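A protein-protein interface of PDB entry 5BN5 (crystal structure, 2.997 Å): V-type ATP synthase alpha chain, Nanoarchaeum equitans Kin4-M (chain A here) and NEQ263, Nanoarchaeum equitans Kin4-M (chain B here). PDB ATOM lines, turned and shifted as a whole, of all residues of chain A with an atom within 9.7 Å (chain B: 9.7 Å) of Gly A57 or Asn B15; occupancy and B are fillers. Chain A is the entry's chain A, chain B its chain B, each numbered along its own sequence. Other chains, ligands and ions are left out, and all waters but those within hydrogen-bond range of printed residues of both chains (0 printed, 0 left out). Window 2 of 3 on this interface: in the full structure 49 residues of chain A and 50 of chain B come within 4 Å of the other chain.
O of Ile A5 lies within hydrogen-bond range of N of Glu B36 (2.9 Å).
N of Ile A7 is in hydrogen-bond range of O of Ala B34.
O of Leu B18 is in hydrogen-bond range of N of Gly A53.
O of Gly A53 lies close to SD of Met B17 (3.5 Å).
O of Ile A4 sits close to O of Val A56 (2.7 Å).
The backbone carbonyl oxygen (O) of Ile A13 sits at hydrogen-bond distance from the backbone NH (N) of Ile A5.
The backbone NH (N) of Ile A13 sits at hydrogen-bond distance from the backbone carbonyl oxygen (O) of Ser A6.
N of Lys A55 lies within hydrogen-bond range of OE1 of Glu A58, 3.1 Å away.
The backbone carbonyl oxygen (O) of Asn B15 sits at hydrogen-bond distance from the guanidinium group (NH2) of Arg B56 (3.0 Å).
N of Met B17 is in hydrogen-bond range of OE2 of Glu B20 (3.1 Å).
Ile A5 touches Tyr B35 (O to CD1, 3.2 Å).
Ser A6 touches Tyr B35 (CB to CD1, 3.5 Å).
Ile A7 touches Leu B18.
O of Leu A54 touches CA of Met B17, at 3.7 Å.
Leu B18 touches Leu A54 (N to O, 3.7 Å).
CA of Lys A55 touches O of Pro B16, at 3.8 Å.
Lys A55 touches Met B17 (NZ to CE, 3.3 Å).
Val A56 touches Pro B16 (CG2 to O, 3.4 Å).
Glu B36 touches Val A56.
Asn B15 touches Gly A57 (CB to N, 3.9 Å).
Of the printed residues of chain B, Ser A6 touches Ala B34 (3.6 Å) and Tyr B35 (3.5 Å).
Printed residues of chain B within 4 Å of Leu A54: Met B17 and Leu B18.
Of chain B, only Asn B15 (3.6 Å), Pro B16 (3.4 Å) and Glu B36 (3.97 Å) come within 4 Å of Val A56.
Of chain B, only Asn B15 (3.9 Å) comes within 4 Å of Gly A57.
Of the printed residues of chain A, Pro B16 touches Lys A55 and Val A56.
Ile B22 touches none of the printed residues of chain A.
Val B31 touches none of the printed residues of chain A.
The nearest residue of chain B that does not touch Gly A57 is Pro B16 (5.6 Å).
The nearest printed residue of chain A that does not touch Tyr B35 is Ile A13 (4.7 Å).
Of the 21 printed residues of chain A, 8 touch a printed residue of chain B.
Of the 20 printed residues of chain B, 7 touch a printed residue of chain A.
Hydrophobic or aromatic side chains of chain B within 4 Å of the printed part of chain A: Pro B16, Met B17, Leu B18 and Tyr B35.
Among the printed residues, 16 pairs touch across the chains.
Among the printed residues, no Asp or Glu carboxylate lies within 4 Å of a Lys or Arg side-chain nitrogen of the other chain.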
ATOM      1  N   MET A   1       1.607  23.763  -4.506  1.00  0.00           N
ATOM      2  CA  MET A   1       1.282  22.343  -4.555  1.00  0.00           C
ATOM      3  C   MET A   1       2.520  21.501  -4.849  1.00  0.00           C
ATOM      4  O   MET A   1       2.760  20.487  -4.195  1.00  0.00           O
ATOM      5  CB  MET A   1       0.202  22.082  -5.595  1.00  0.00           C
ATOM      6  N   ASN A   2       3.299  21.928  -5.837  1.00  0.00           N
ATOM      7  CA  ASN A   2       4.516  21.219  -6.215  1.00  0.00           C
ATOM      8  C   ASN A   2       5.576  21.287  -5.122  1.00  0.00           C
ATOM      9  O   ASN A   2       5.698  22.295  -4.427  1.00  0.00           O
ATOM     10  CB  ASN A   2       5.079  21.776  -7.524  1.00  0.00           C
ATOM     11  CG  ASN A   2       4.079  21.714  -8.661  1.00  0.00           C
ATOM     12  OD1 ASN A   2       3.190  20.863  -8.676  1.00  0.00           O
ATOM     13  ND2 ASN A   2       4.221  22.618  -9.623  1.00  0.00           N
ATOM     14  N   ARG A   3       6.341  20.210  -4.975  1.00  0.00           N
ATOM     15  CA  ARG A   3       7.377  20.143  -3.952  1.00  0.00           C
ATOM     16  C   ARG A   3       8.483  19.164  -4.330  1.00  0.00           C
ATOM     17  O   ARG A   3       8.220  18.094  -4.876  1.00  0.00           O
ATOM     18  CB  ARG A   3       6.770  19.766  -2.607  1.00  0.00           C
ATOM     19  N   ILE A   4       9.723  19.541  -4.033  1.00  0.00           N
ATOM     20  CA  ILE A   4      10.877  18.691  -4.294  1.00  0.00           C
ATOM     21  C   ILE A   4      10.867  17.484  -3.360  1.00  0.00           C
ATOM     22  O   ILE A   4      10.525  17.604  -2.187  1.00  0.00           O
ATOM     23  CB  ILE A   4      12.192  19.473  -4.098  1.00  0.00           C
ATOM     24  CG1 ILE A   4      12.201  20.730  -4.970  1.00  0.00           C
ATOM     25  CG2 ILE A   4      13.399  18.599  -4.407  1.00  0.00           C
ATOM     26  CD1 ILE A   4      13.452  21.567  -4.821  1.00  0.00           C
ATOM     27  N   ILE A   5      11.230  16.318  -3.885  1.00  0.00           N
ATOM     28  CA  ILE A   5      11.325  15.118  -3.061  1.00  0.00           C
ATOM     29  C   ILE A   5      12.754  14.588  -3.008  1.00  0.00           C
ATOM     30  O   ILE A   5      13.106  13.821  -2.111  1.00  0.00           O
ATOM     31  CB  ILE A   5      10.391  14.000  -3.561  1.00  0.00           C
ATOM     32  CG1 ILE A   5      10.759  13.591  -4.988  1.00  0.00           C
ATOM     33  CG2 ILE A   5       8.939  14.443  -3.483  1.00  0.00           C
ATOM     34  CD1 ILE A   5       9.987  12.397  -5.493  1.00  0.00           C
ATOM     35  N   SER A   6      13.574  15.001  -3.969  1.00  0.00           N
ATOM     36  CA  SER A   6      14.955  14.540  -4.037  1.00  0.00           C
ATOM     37  C   SER A   6      15.863  15.549  -4.730  1.00  0.00           C
ATOM     38  O   SER A   6      15.494  16.143  -5.744  1.00  0.00           O
ATOM     39  CB  SER A   6      15.035  13.192  -4.752  1.00  0.00           C
ATOM     40  OG  SER A   6      16.373  12.732  -4.825  1.00  0.00           O
ATOM     41  N   ILE A   7      17.054  15.738  -4.172  1.00  0.00           N
ATOM     42  CA  ILE A   7      18.048  16.631  -4.753  1.00  0.00           C
ATOM     43  C   ILE A   7      19.358  15.880  -4.957  1.00  0.00           C
ATOM     44  O   ILE A   7      19.961  15.398  -4.000  1.00  0.00           O
ATOM     45  CB  ILE A   7      18.306  17.850  -3.851  1.00  0.00           C
ATOM     46  CG1 ILE A   7      16.988  18.544  -3.499  1.00  0.00           C
ATOM     47  CG2 ILE A   7      19.264  18.819  -4.529  1.00  0.00           C
ATOM     48  CD1 ILE A   7      17.138  19.674  -2.508  1.00  0.00           C
ATOM     49  N   ILE A  13      14.425  16.160  -8.254  1.00  0.00           N
ATOM     50  CA  ILE A  13      13.156  15.465  -8.443  1.00  0.00           C
ATOM     51  C   ILE A  13      12.044  16.138  -7.646  1.00  0.00           C
ATOM     52  O   ILE A  13      12.155  16.307  -6.432  1.00  0.00           O
ATOM     53  CB  ILE A  13      13.256  13.988  -8.022  1.00  0.00           C
ATOM     54  CG1 ILE A  13      14.529  13.354  -8.588  1.00  0.00           C
ATOM     55  CG2 ILE A  13      12.022  13.222  -8.471  1.00  0.00           C
ATOM     56  CD1 ILE A  13      14.732  11.914  -8.169  1.00  0.00           C
ATOM     57  N   VAL A  26      12.873  26.473  -9.514  1.00  0.00           N
ATOM     58  CA  VAL A  26      13.162  25.597  -8.383  1.00  0.00           C
ATOM     59  C   VAL A  26      13.341  26.354  -7.068  1.00  0.00           C
ATOM     60  O   VAL A  26      14.115  27.308  -6.988  1.00  0.00           O
ATOM     61  CB  VAL A  26      14.424  24.751  -8.650  1.00  0.00           C
ATOM     62  CG1 VAL A  26      14.711  23.830  -7.473  1.00  0.00           C
ATOM     63  CG2 VAL A  26      14.262  23.949  -9.932  1.00  0.00           C
ATOM     64  N   GLY A  27      12.617  25.916  -6.041  1.00  0.00           N
ATOM     65  CA  GLY A  27      12.755  26.472  -4.707  1.00  0.00           C
ATOM     66  C   GLY A  27      12.122  27.839  -4.544  1.00  0.00           C
ATOM     67  O   GLY A  27      11.524  28.375  -5.478  1.00  0.00           O
ATOM     68  N   GLU A  28      12.254  28.403  -3.348  1.00  0.00           N
ATOM     69  CA  GLU A  28      11.749  29.742  -3.069  1.00  0.00           C
ATOM     70  C   GLU A  28      12.685  30.790  -3.660  1.00  0.00           C
ATOM     71  O   GLU A  28      12.343  31.968  -3.747  1.00  0.00           O
ATOM     72  CB  GLU A  28      11.593  29.950  -1.571  1.00  0.00           C
ATOM     73  N   GLU A  29      13.871  30.345  -4.064  1.00  0.00           N
ATOM     74  CA  GLU A  29      14.850  31.218  -4.695  1.00  0.00           C
ATOM     75  C   GLU A  29      14.586  31.278  -6.197  1.00  0.00           C
ATOM     76  O   GLU A  29      15.196  32.071  -6.916  1.00  0.00           O
ATOM     77  CB  GLU A  29      16.266  30.710  -4.414  1.00  0.00           C
ATOM     78  CG  GLU A  29      17.361  31.751  -4.588  1.00  0.00           C
ATOM     79  CD  GLU A  29      18.704  31.276  -4.065  1.00  0.00           C
ATOM     80  OE1 GLU A  29      18.792  30.111  -3.621  1.00  0.00           O
ATOM     81  OE2 GLU A  29      19.670  32.067  -4.093  1.00  0.00           O
ATOM     82  N   GLY A  53      22.177  23.654  -1.146  1.00  0.00           N
ATOM     83  CA  GLY A  53      21.557  24.438  -0.094  1.00  0.00           C
ATOM     84  C   GLY A  53      20.043  24.397  -0.164  1.00  0.00           C
ATOM     85  O   GLY A  53      19.357  24.913   0.717  1.00  0.00           O
ATOM     86  N   LEU A  54      19.524  23.779  -1.220  1.00  0.00           N
ATOM     87  CA  LEU A  54      18.083  23.675  -1.416  1.00  0.00           C
ATOM     88  C   LEU A  54      17.456  22.697  -0.429  1.00  0.00           C
ATOM     89  O   LEU A  54      18.069  21.699  -0.050  1.00  0.00           O
ATOM     90  CB  LEU A  54      17.767  23.246  -2.851  1.00  0.00           C
ATOM     91  CG  LEU A  54      18.249  24.177  -3.965  1.00  0.00           C
ATOM     92  CD1 LEU A  54      17.819  23.645  -5.324  1.00  0.00           C
ATOM     93  CD2 LEU A  54      17.733  25.592  -3.750  1.00  0.00           C
ATOM     94  N   LYS A  55      16.228  22.992  -0.016  1.00  0.00           N
ATOM     95  CA  LYS A  55      15.514  22.148   0.933  1.00  0.00           C
ATOM     96  C   LYS A  55      14.587  21.183   0.205  1.00  0.00           C
ATOM     97  O   LYS A  55      14.300  21.355  -0.980  1.00  0.00           O
ATOM     98  CB  LYS A  55      14.697  23.007   1.901  1.00  0.00           C
ATOM     99  CG  LYS A  55      15.475  24.134   2.559  1.00  0.00           C
ATOM    100  CD  LYS A  55      14.545  25.043   3.350  1.00  0.00           C
ATOM    101  CE  LYS A  55      15.288  26.229   3.941  1.00  0.00           C
ATOM    102  NZ  LYS A  55      16.298  25.809   4.950  1.00  0.00           N
ATOM    103  N   VAL A  56      14.120  20.167   0.923  1.00  0.00           N
ATOM    104  CA  VAL A  56      13.145  19.232   0.380  1.00  0.00           C
ATOM    105  C   VAL A  56      11.752  19.847   0.501  1.00  0.00           C
ATOM    106  O   VAL A  56      10.837  19.506  -0.247  1.00  0.00           O
ATOM    107  CB  VAL A  56      13.201  17.877   1.115  1.00  0.00           C
ATOM    108  CG1 VAL A  56      12.313  16.849   0.428  1.00  0.00           C
ATOM    109  CG2 VAL A  56      14.633  17.375   1.178  1.00  0.00           C
ATOM    110  N   GLY A  57      11.606  20.775   1.440  1.00  0.00           N
ATOM    111  CA  GLY A  57      10.345  21.466   1.639  1.00  0.00           C
ATOM    112  C   GLY A  57      10.217  22.714   0.784  1.00  0.00           C
ATOM    113  O   GLY A  57       9.541  23.670   1.164  1.00  0.00           O
ATOM    114  N   GLU A  58      10.868  22.705  -0.376  1.00  0.00           N
ATOM    115  CA  GLU A  58      10.811  23.834  -1.297  1.00  0.00           C
ATOM    116  C   GLU A  58       9.940  23.526  -2.512  1.00  0.00           C
ATOM    117  O   GLU A  58       9.991  22.421  -3.053  1.00  0.00           O
ATOM    118  CB  GLU A  58      12.217  24.243  -1.740  1.00  0.00           C
ATOM    119  CG  GLU A  58      13.020  24.958  -0.669  1.00  0.00           C
ATOM    120  CD  GLU A  58      14.400  25.362  -1.147  1.00  0.00           C
ATOM    121  OE1 GLU A  58      14.875  24.785  -2.148  1.00  0.00           O
ATOM    122  OE2 GLU A  58      15.008  26.258  -0.525  1.00  0.00           O
ATOM    123  N   PRO A  59       9.137  24.510  -2.943  1.00  0.00           N
ATOM    124  CA  PRO A  59       8.208  24.349  -4.066  1.00  0.00           C
ATOM    125  C   PRO A  59       8.882  24.532  -5.424  1.00  0.00           C
ATOM    126  O   PRO A  59      10.018  24.999  -5.499  1.00  0.00           O
ATOM    127  CB  PRO A  59       7.202  25.476  -3.835  1.00  0.00           C
ATOM    128  CG  PRO A  59       8.009  26.547  -3.190  1.00  0.00           C
ATOM    129  CD  PRO A  59       9.015  25.840  -2.316  1.00  0.00           C
ATOM    130  N   VAL A  60       8.174  24.158  -6.485  1.00  0.00           N
ATOM    131  CA  VAL A  60       8.659  24.338  -7.848  1.00  0.00           C
ATOM    132  C   VAL A  60       7.557  24.939  -8.716  1.00  0.00           C
ATOM    133  O   VAL A  60       6.498  24.337  -8.894  1.00  0.00           O
ATOM    134  CB  VAL A  60       9.132  23.006  -8.465  1.00  0.00           C
ATOM    135  CG1 VAL A  60       9.387  23.171  -9.953  1.00  0.00           C
ATOM    136  CG2 VAL A  60      10.382  22.502  -7.756  1.00  0.00           C
ATOM    137  N   PHE A  61       7.810  26.128  -9.253  1.00  0.00           N
ATOM    138  CA  PHE A  61       6.796  26.854 -10.011  1.00  0.00           C
ATOM    139  C   PHE A  61       6.792  26.473 -11.489  1.00  0.00           C
ATOM    140  O   PHE A  61       7.796  26.002 -12.022  1.00  0.00           O
ATOM    141  CB  PHE A  61       7.000  28.362  -9.857  1.00  0.00           C
ATOM    142  CG  PHE A  61       7.185  28.804  -8.433  1.00  0.00           C
ATOM    143  CD1 PHE A  61       6.097  28.928  -7.585  1.00  0.00           C
ATOM    144  CD2 PHE A  61       8.447  29.096  -7.943  1.00  0.00           C
ATOM    145  CE1 PHE A  61       6.264  29.333  -6.275  1.00  0.00           C
ATOM    146  CE2 PHE A  61       8.621  29.502  -6.634  1.00  0.00           C
ATOM    147  CZ  PHE A  61       7.528  29.621  -5.799  1.00  0.00           C
ATOM    148  N   VAL B  11      20.966   9.018   8.467  1.00  0.00           N
ATOM    149  CA  VAL B  11      20.182   9.758   9.450  1.00  0.00           C
ATOM    150  C   VAL B  11      18.814  10.191   8.916  1.00  0.00           C
ATOM    151  O   VAL B  11      18.694  10.642   7.776  1.00  0.00           O
ATOM    152  CB  VAL B  11      20.970  10.987   9.966  1.00  0.00           C
ATOM    153  CG1 VAL B  11      21.446  11.850   8.803  1.00  0.00           C
ATOM    154  CG2 VAL B  11      20.134  11.799  10.941  1.00  0.00           C
ATOM    155  N   GLU B  12      17.786  10.038   9.745  1.00  0.00           N
ATOM    156  CA  GLU B  12      16.440  10.471   9.392  1.00  0.00           C
ATOM    157  C   GLU B  12      16.256  11.944   9.745  1.00  0.00           C
ATOM    158  O   GLU B  12      16.284  12.316  10.918  1.00  0.00           O
ATOM    159  CB  GLU B  12      15.389   9.633  10.127  1.00  0.00           C
ATOM    160  CG  GLU B  12      15.760   8.170  10.325  1.00  0.00           C
ATOM    161  CD  GLU B  12      16.549   7.933  11.600  1.00  0.00           C
ATOM    162  OE1 GLU B  12      16.897   8.923  12.279  1.00  0.00           O
ATOM    163  OE2 GLU B  12      16.818   6.758  11.926  1.00  0.00           O
ATOM    164  N   LEU B  13      16.069  12.779   8.729  1.00  0.00           N
ATOM    165  CA  LEU B  13      15.894  14.212   8.943  1.00  0.00           C
ATOM    166  C   LEU B  13      14.667  14.744   8.209  1.00  0.00           C
ATOM    167  O   LEU B  13      14.440  14.417   7.045  1.00  0.00           O
ATOM    168  CB  LEU B  13      17.143  14.978   8.498  1.00  0.00           C
ATOM    169  CG  LEU B  13      18.435  14.691   9.266  1.00  0.00           C
ATOM    170  CD1 LEU B  13      19.598  15.470   8.670  1.00  0.00           C
ATOM    171  CD2 LEU B  13      18.267  15.020  10.741  1.00  0.00           C
ATOM    172  N   GLU B  14      13.882  15.565   8.897  1.00  0.00           N
ATOM    173  CA  GLU B  14      12.688  16.161   8.307  1.00  0.00           C
ATOM    174  C   GLU B  14      13.060  17.204   7.259  1.00  0.00           C
ATOM    175  O   GLU B  14      13.414  18.334   7.597  1.00  0.00           O
ATOM    176  CB  GLU B  14      11.813  16.779   9.387  1.00  0.00           C
ATOM    177  N   ASN B  15      12.974  16.810   5.990  1.00  0.00           N
ATOM    178  CA  ASN B  15      13.346  17.669   4.866  1.00  0.00           C
ATOM    179  C   ASN B  15      14.762  18.235   4.985  1.00  0.00           C
ATOM    180  O   ASN B  15      14.939  19.411   5.304  1.00  0.00           O
ATOM    181  CB  ASN B  15      12.331  18.802   4.687  1.00  0.00           C
ATOM    182  CG  ASN B  15      10.943  18.291   4.352  1.00  0.00           C
ATOM    183  OD1 ASN B  15      10.790  17.285   3.659  1.00  0.00           O
ATOM    184  ND2 ASN B  15       9.923  18.984   4.844  1.00  0.00           N
ATOM    185  N   PRO B  16      15.776  17.392   4.725  1.00  0.00           N
ATOM    186  CA  PRO B  16      17.186  17.776   4.856  1.00  0.00           C
ATOM    187  C   PRO B  16      17.627  18.811   3.823  1.00  0.00           C
ATOM    188  O   PRO B  16      16.819  19.292   3.028  1.00  0.00           O
ATOM    189  CB  PRO B  16      17.934  16.458   4.614  1.00  0.00           C
ATOM    190  CG  PRO B  16      16.919  15.384   4.835  1.00  0.00           C
ATOM    191  CD  PRO B  16      15.628  15.971   4.374  1.00  0.00           C
ATOM    192  N   MET B  17      18.915  19.140   3.847  1.00  0.00           N
ATOM    193  CA  MET B  17      19.493  20.102   2.919  1.00  0.00           C
ATOM    194  C   MET B  17      20.814  19.570   2.376  1.00  0.00           C
ATOM    195  O   MET B  17      21.583  18.943   3.104  1.00  0.00           O
ATOM    196  CB  MET B  17      19.713  21.446   3.618  1.00  0.00           C
ATOM    197  CG  MET B  17      20.495  22.462   2.802  1.00  0.00           C
ATOM    198  SD  MET B  17      20.900  23.952   3.733  1.00  0.00           S
ATOM    199  CE  MET B  17      19.263  24.592   4.069  1.00  0.00           C
ATOM    200  N   LEU B  18      21.072  19.812   1.095  1.00  0.00           N
ATOM    201  CA  LEU B  18      22.324  19.386   0.478  1.00  0.00           C
ATOM    202  C   LEU B  18      23.490  20.202   1.029  1.00  0.00           C
ATOM    203  O   LEU B  18      23.512  21.427   0.909  1.00  0.00           O
ATOM    204  CB  LEU B  18      22.251  19.531  -1.043  1.00  0.00           C
ATOM    205  CG  LEU B  18      22.773  18.358  -1.878  1.00  0.00           C
ATOM    206  CD1 LEU B  18      22.774  18.712  -3.358  1.00  0.00           C
ATOM    207  CD2 LEU B  18      24.159  17.920  -1.426  1.00  0.00           C
ATOM    208  N   GLU B  20      24.247  20.352   4.190  1.00  0.00           N
ATOM    209  CA  GLU B  20      23.845  20.881   5.489  1.00  0.00           C
ATOM    210  C   GLU B  20      24.795  20.430   6.593  1.00  0.00           C
ATOM    211  O   GLU B  20      25.239  19.283   6.614  1.00  0.00           O
ATOM    212  CB  GLU B  20      22.415  20.448   5.822  1.00  0.00           C
ATOM    213  CG  GLU B  20      21.867  21.035   7.114  1.00  0.00           C
ATOM    214  CD  GLU B  20      20.477  20.529   7.444  1.00  0.00           C
ATOM    215  OE1 GLU B  20      19.872  21.038   8.412  1.00  0.00           O
ATOM    216  OE2 GLU B  20      19.987  19.623   6.737  1.00  0.00           O
ATOM    217  N   ILE B  22      25.402  19.470  10.404  1.00  0.00           N
ATOM    218  CA  ILE B  22      24.682  18.996  11.579  1.00  0.00           C
ATOM    219  C   ILE B  22      25.615  18.798  12.772  1.00  0.00           C
ATOM    220  O   ILE B  22      26.500  17.943  12.751  1.00  0.00           O
ATOM    221  CB  ILE B  22      23.914  17.692  11.286  1.00  0.00           C
ATOM    222  CG1 ILE B  22      24.758  16.758  10.417  1.00  0.00           C
ATOM    223  CG2 ILE B  22      22.601  18.001  10.587  1.00  0.00           C
ATOM    224  CD1 ILE B  22      24.072  15.454  10.075  1.00  0.00           C
ATOM    225  N   VAL B  31      25.765  16.827   5.420  1.00  0.00           N
ATOM    226  CA  VAL B  31      24.733  16.063   4.728  1.00  0.00           C
ATOM    227  C   VAL B  31      24.983  16.068   3.223  1.00  0.00           C
ATOM    228  O   VAL B  31      24.777  17.080   2.553  1.00  0.00           O
ATOM    229  CB  VAL B  31      23.329  16.631   5.014  1.00  0.00           C
ATOM    230  CG1 VAL B  31      22.269  15.818   4.288  1.00  0.00           C
ATOM    231  CG2 VAL B  31      23.062  16.650   6.512  1.00  0.00           C
ATOM    232  N   ALA B  33      23.795  13.483   1.017  1.00  0.00           N
ATOM    233  CA  ALA B  33      22.688  12.878   0.285  1.00  0.00           C
ATOM    234  C   ALA B  33      21.349  13.322   0.863  1.00  0.00           C
ATOM    235  O   ALA B  33      21.258  13.661   2.041  1.00  0.00           O
ATOM    236  CB  ALA B  33      22.802  11.362   0.307  1.00  0.00           C
ATOM    237  N   ALA B  34      20.312  13.315   0.030  1.00  0.00           N
ATOM    238  CA  ALA B  34      18.989  13.753   0.463  1.00  0.00           C
ATOM    239  C   ALA B  34      17.864  13.185  -0.400  1.00  0.00           C
ATOM    240  O   ALA B  34      17.706  13.564  -1.560  1.00  0.00           O
ATOM    241  CB  ALA B  34      18.918  15.275   0.490  1.00  0.00           C
ATOM    242  N   TYR B  35      17.086  12.276   0.178  1.00  0.00           N
ATOM    243  CA  TYR B  35      15.890  11.753  -0.474  1.00  0.00           C
ATOM    244  C   TYR B  35      14.771  11.649   0.557  1.00  0.00           C
ATOM    245  O   TYR B  35      14.867  10.876   1.511  1.00  0.00           O
ATOM    246  CB  TYR B  35      16.165  10.385  -1.108  1.00  0.00           C
ATOM    247  CG  TYR B  35      15.191   9.998  -2.205  1.00  0.00           C
ATOM    248  CD1 TYR B  35      14.031  10.730  -2.429  1.00  0.00           C
ATOM    249  CD2 TYR B  35      15.435   8.897  -3.018  1.00  0.00           C
ATOM    250  CE1 TYR B  35      13.143  10.379  -3.429  1.00  0.00           C
ATOM    251  CE2 TYR B  35      14.551   8.538  -4.020  1.00  0.00           C
ATOM    252  CZ  TYR B  35      13.408   9.283  -4.221  1.00  0.00           C
ATOM    253  OH  TYR B  35      12.524   8.931  -5.217  1.00  0.00           O
ATOM    254  N   GLU B  36      13.714  12.433   0.351  1.00  0.00           N
ATOM    255  CA  GLU B  36      12.594  12.514   1.287  1.00  0.00           C
ATOM    256  C   GLU B  36      13.056  12.873   2.695  1.00  0.00           C
ATOM    257  O   GLU B  36      13.578  13.964   2.925  1.00  0.00           O
ATOM    258  CB  GLU B  36      11.789  11.208   1.301  1.00  0.00           C
ATOM    259  CG  GLU B  36      10.979  10.957   0.038  1.00  0.00           C
ATOM    260  CD  GLU B  36       9.787  11.889  -0.091  1.00  0.00           C
ATOM    261  OE1 GLU B  36       9.424  12.541   0.911  1.00  0.00           O
ATOM    262  OE2 GLU B  36       9.210  11.967  -1.195  1.00  0.00           O
ATOM    263  N   ASN B  37      12.864  11.953   3.633  1.00  0.00           N
ATOM    264  CA  ASN B  37      13.280  12.170   5.012  1.00  0.00           C
ATOM    265  C   ASN B  37      14.505  11.343   5.393  1.00  0.00           C
ATOM    266  O   ASN B  37      14.767  11.109   6.573  1.00  0.00           O
ATOM    267  CB  ASN B  37      12.122  11.897   5.975  1.00  0.00           C
ATOM    268  CG  ASN B  37      11.337  10.656   5.605  1.00  0.00           C
ATOM    269  OD1 ASN B  37      11.820   9.797   4.867  1.00  0.00           O
ATOM    270  ND2 ASN B  37      10.114  10.555   6.117  1.00  0.00           N
ATOM    271  N   LYS B  38      15.251  10.904   4.384  1.00  0.00           N
ATOM    272  CA  LYS B  38      16.478  10.147   4.601  1.00  0.00           C
ATOM    273  C   LYS B  38      17.680  10.925   4.076  1.00  0.00           C
ATOM    274  O   LYS B  38      17.580  11.634   3.075  1.00  0.00           O
ATOM    275  CB  LYS B  38      16.392   8.782   3.916  1.00  0.00           C
ATOM    276  CG  LYS B  38      15.266   7.901   4.431  1.00  0.00           C
ATOM    277  CD  LYS B  38      15.206   6.582   3.679  1.00  0.00           C
ATOM    278  CE  LYS B  38      14.096   5.692   4.214  1.00  0.00           C
ATOM    279  NZ  LYS B  38      12.763   6.348   4.121  1.00  0.00           N
ATOM    280  N   ALA B  39      18.817  10.790   4.753  1.00  0.00           N
ATOM    281  CA  ALA B  39      20.015  11.531   4.376  1.00  0.00           C
ATOM    282  C   ALA B  39      21.299  10.840   4.828  1.00  0.00           C
ATOM    283  O   ALA B  39      21.315  10.136   5.838  1.00  0.00           O
ATOM    284  CB  ALA B  39      19.955  12.947   4.934  1.00  0.00           C
ATOM    285  N   ARG B  56      20.588  20.493  13.842  1.00  0.00           N
ATOM    286  CA  ARG B  56      20.601  20.980  12.467  1.00  0.00           C
ATOM    287  C   ARG B  56      20.742  22.498  12.411  1.00  0.00           C
ATOM    288  O   ARG B  56      19.908  23.227  12.949  1.00  0.00           O
ATOM    289  CB  ARG B  56      19.325  20.547  11.743  1.00  0.00           C
ATOM    290  CG  ARG B  56      19.093  19.044  11.741  1.00  0.00           C
ATOM    291  CD  ARG B  56      17.699  18.700  11.241  1.00  0.00           C
ATOM    292  NE  ARG B  56      17.469  19.176   9.880  1.00  0.00           N
ATOM    293  CZ  ARG B  56      16.327  19.021   9.220  1.00  0.00           C
ATOM    294  NH1 ARG B  56      15.304  18.403   9.795  1.00  0.00           N
ATOM    295  NH2 ARG B  56      16.204  19.485   7.984  1.00  0.00           N
ATOM    296  N   GLY B  58      21.012  24.387   9.418  1.00  0.00           N
ATOM    297  CA  GLY B  58      20.194  24.894   8.332  1.00  0.00           C
ATOM    298  C   GLY B  58      21.025  25.673   7.331  1.00  0.00           C
ATOM    299  O   GLY B  58      20.491  26.428   6.518  1.00  0.00           O
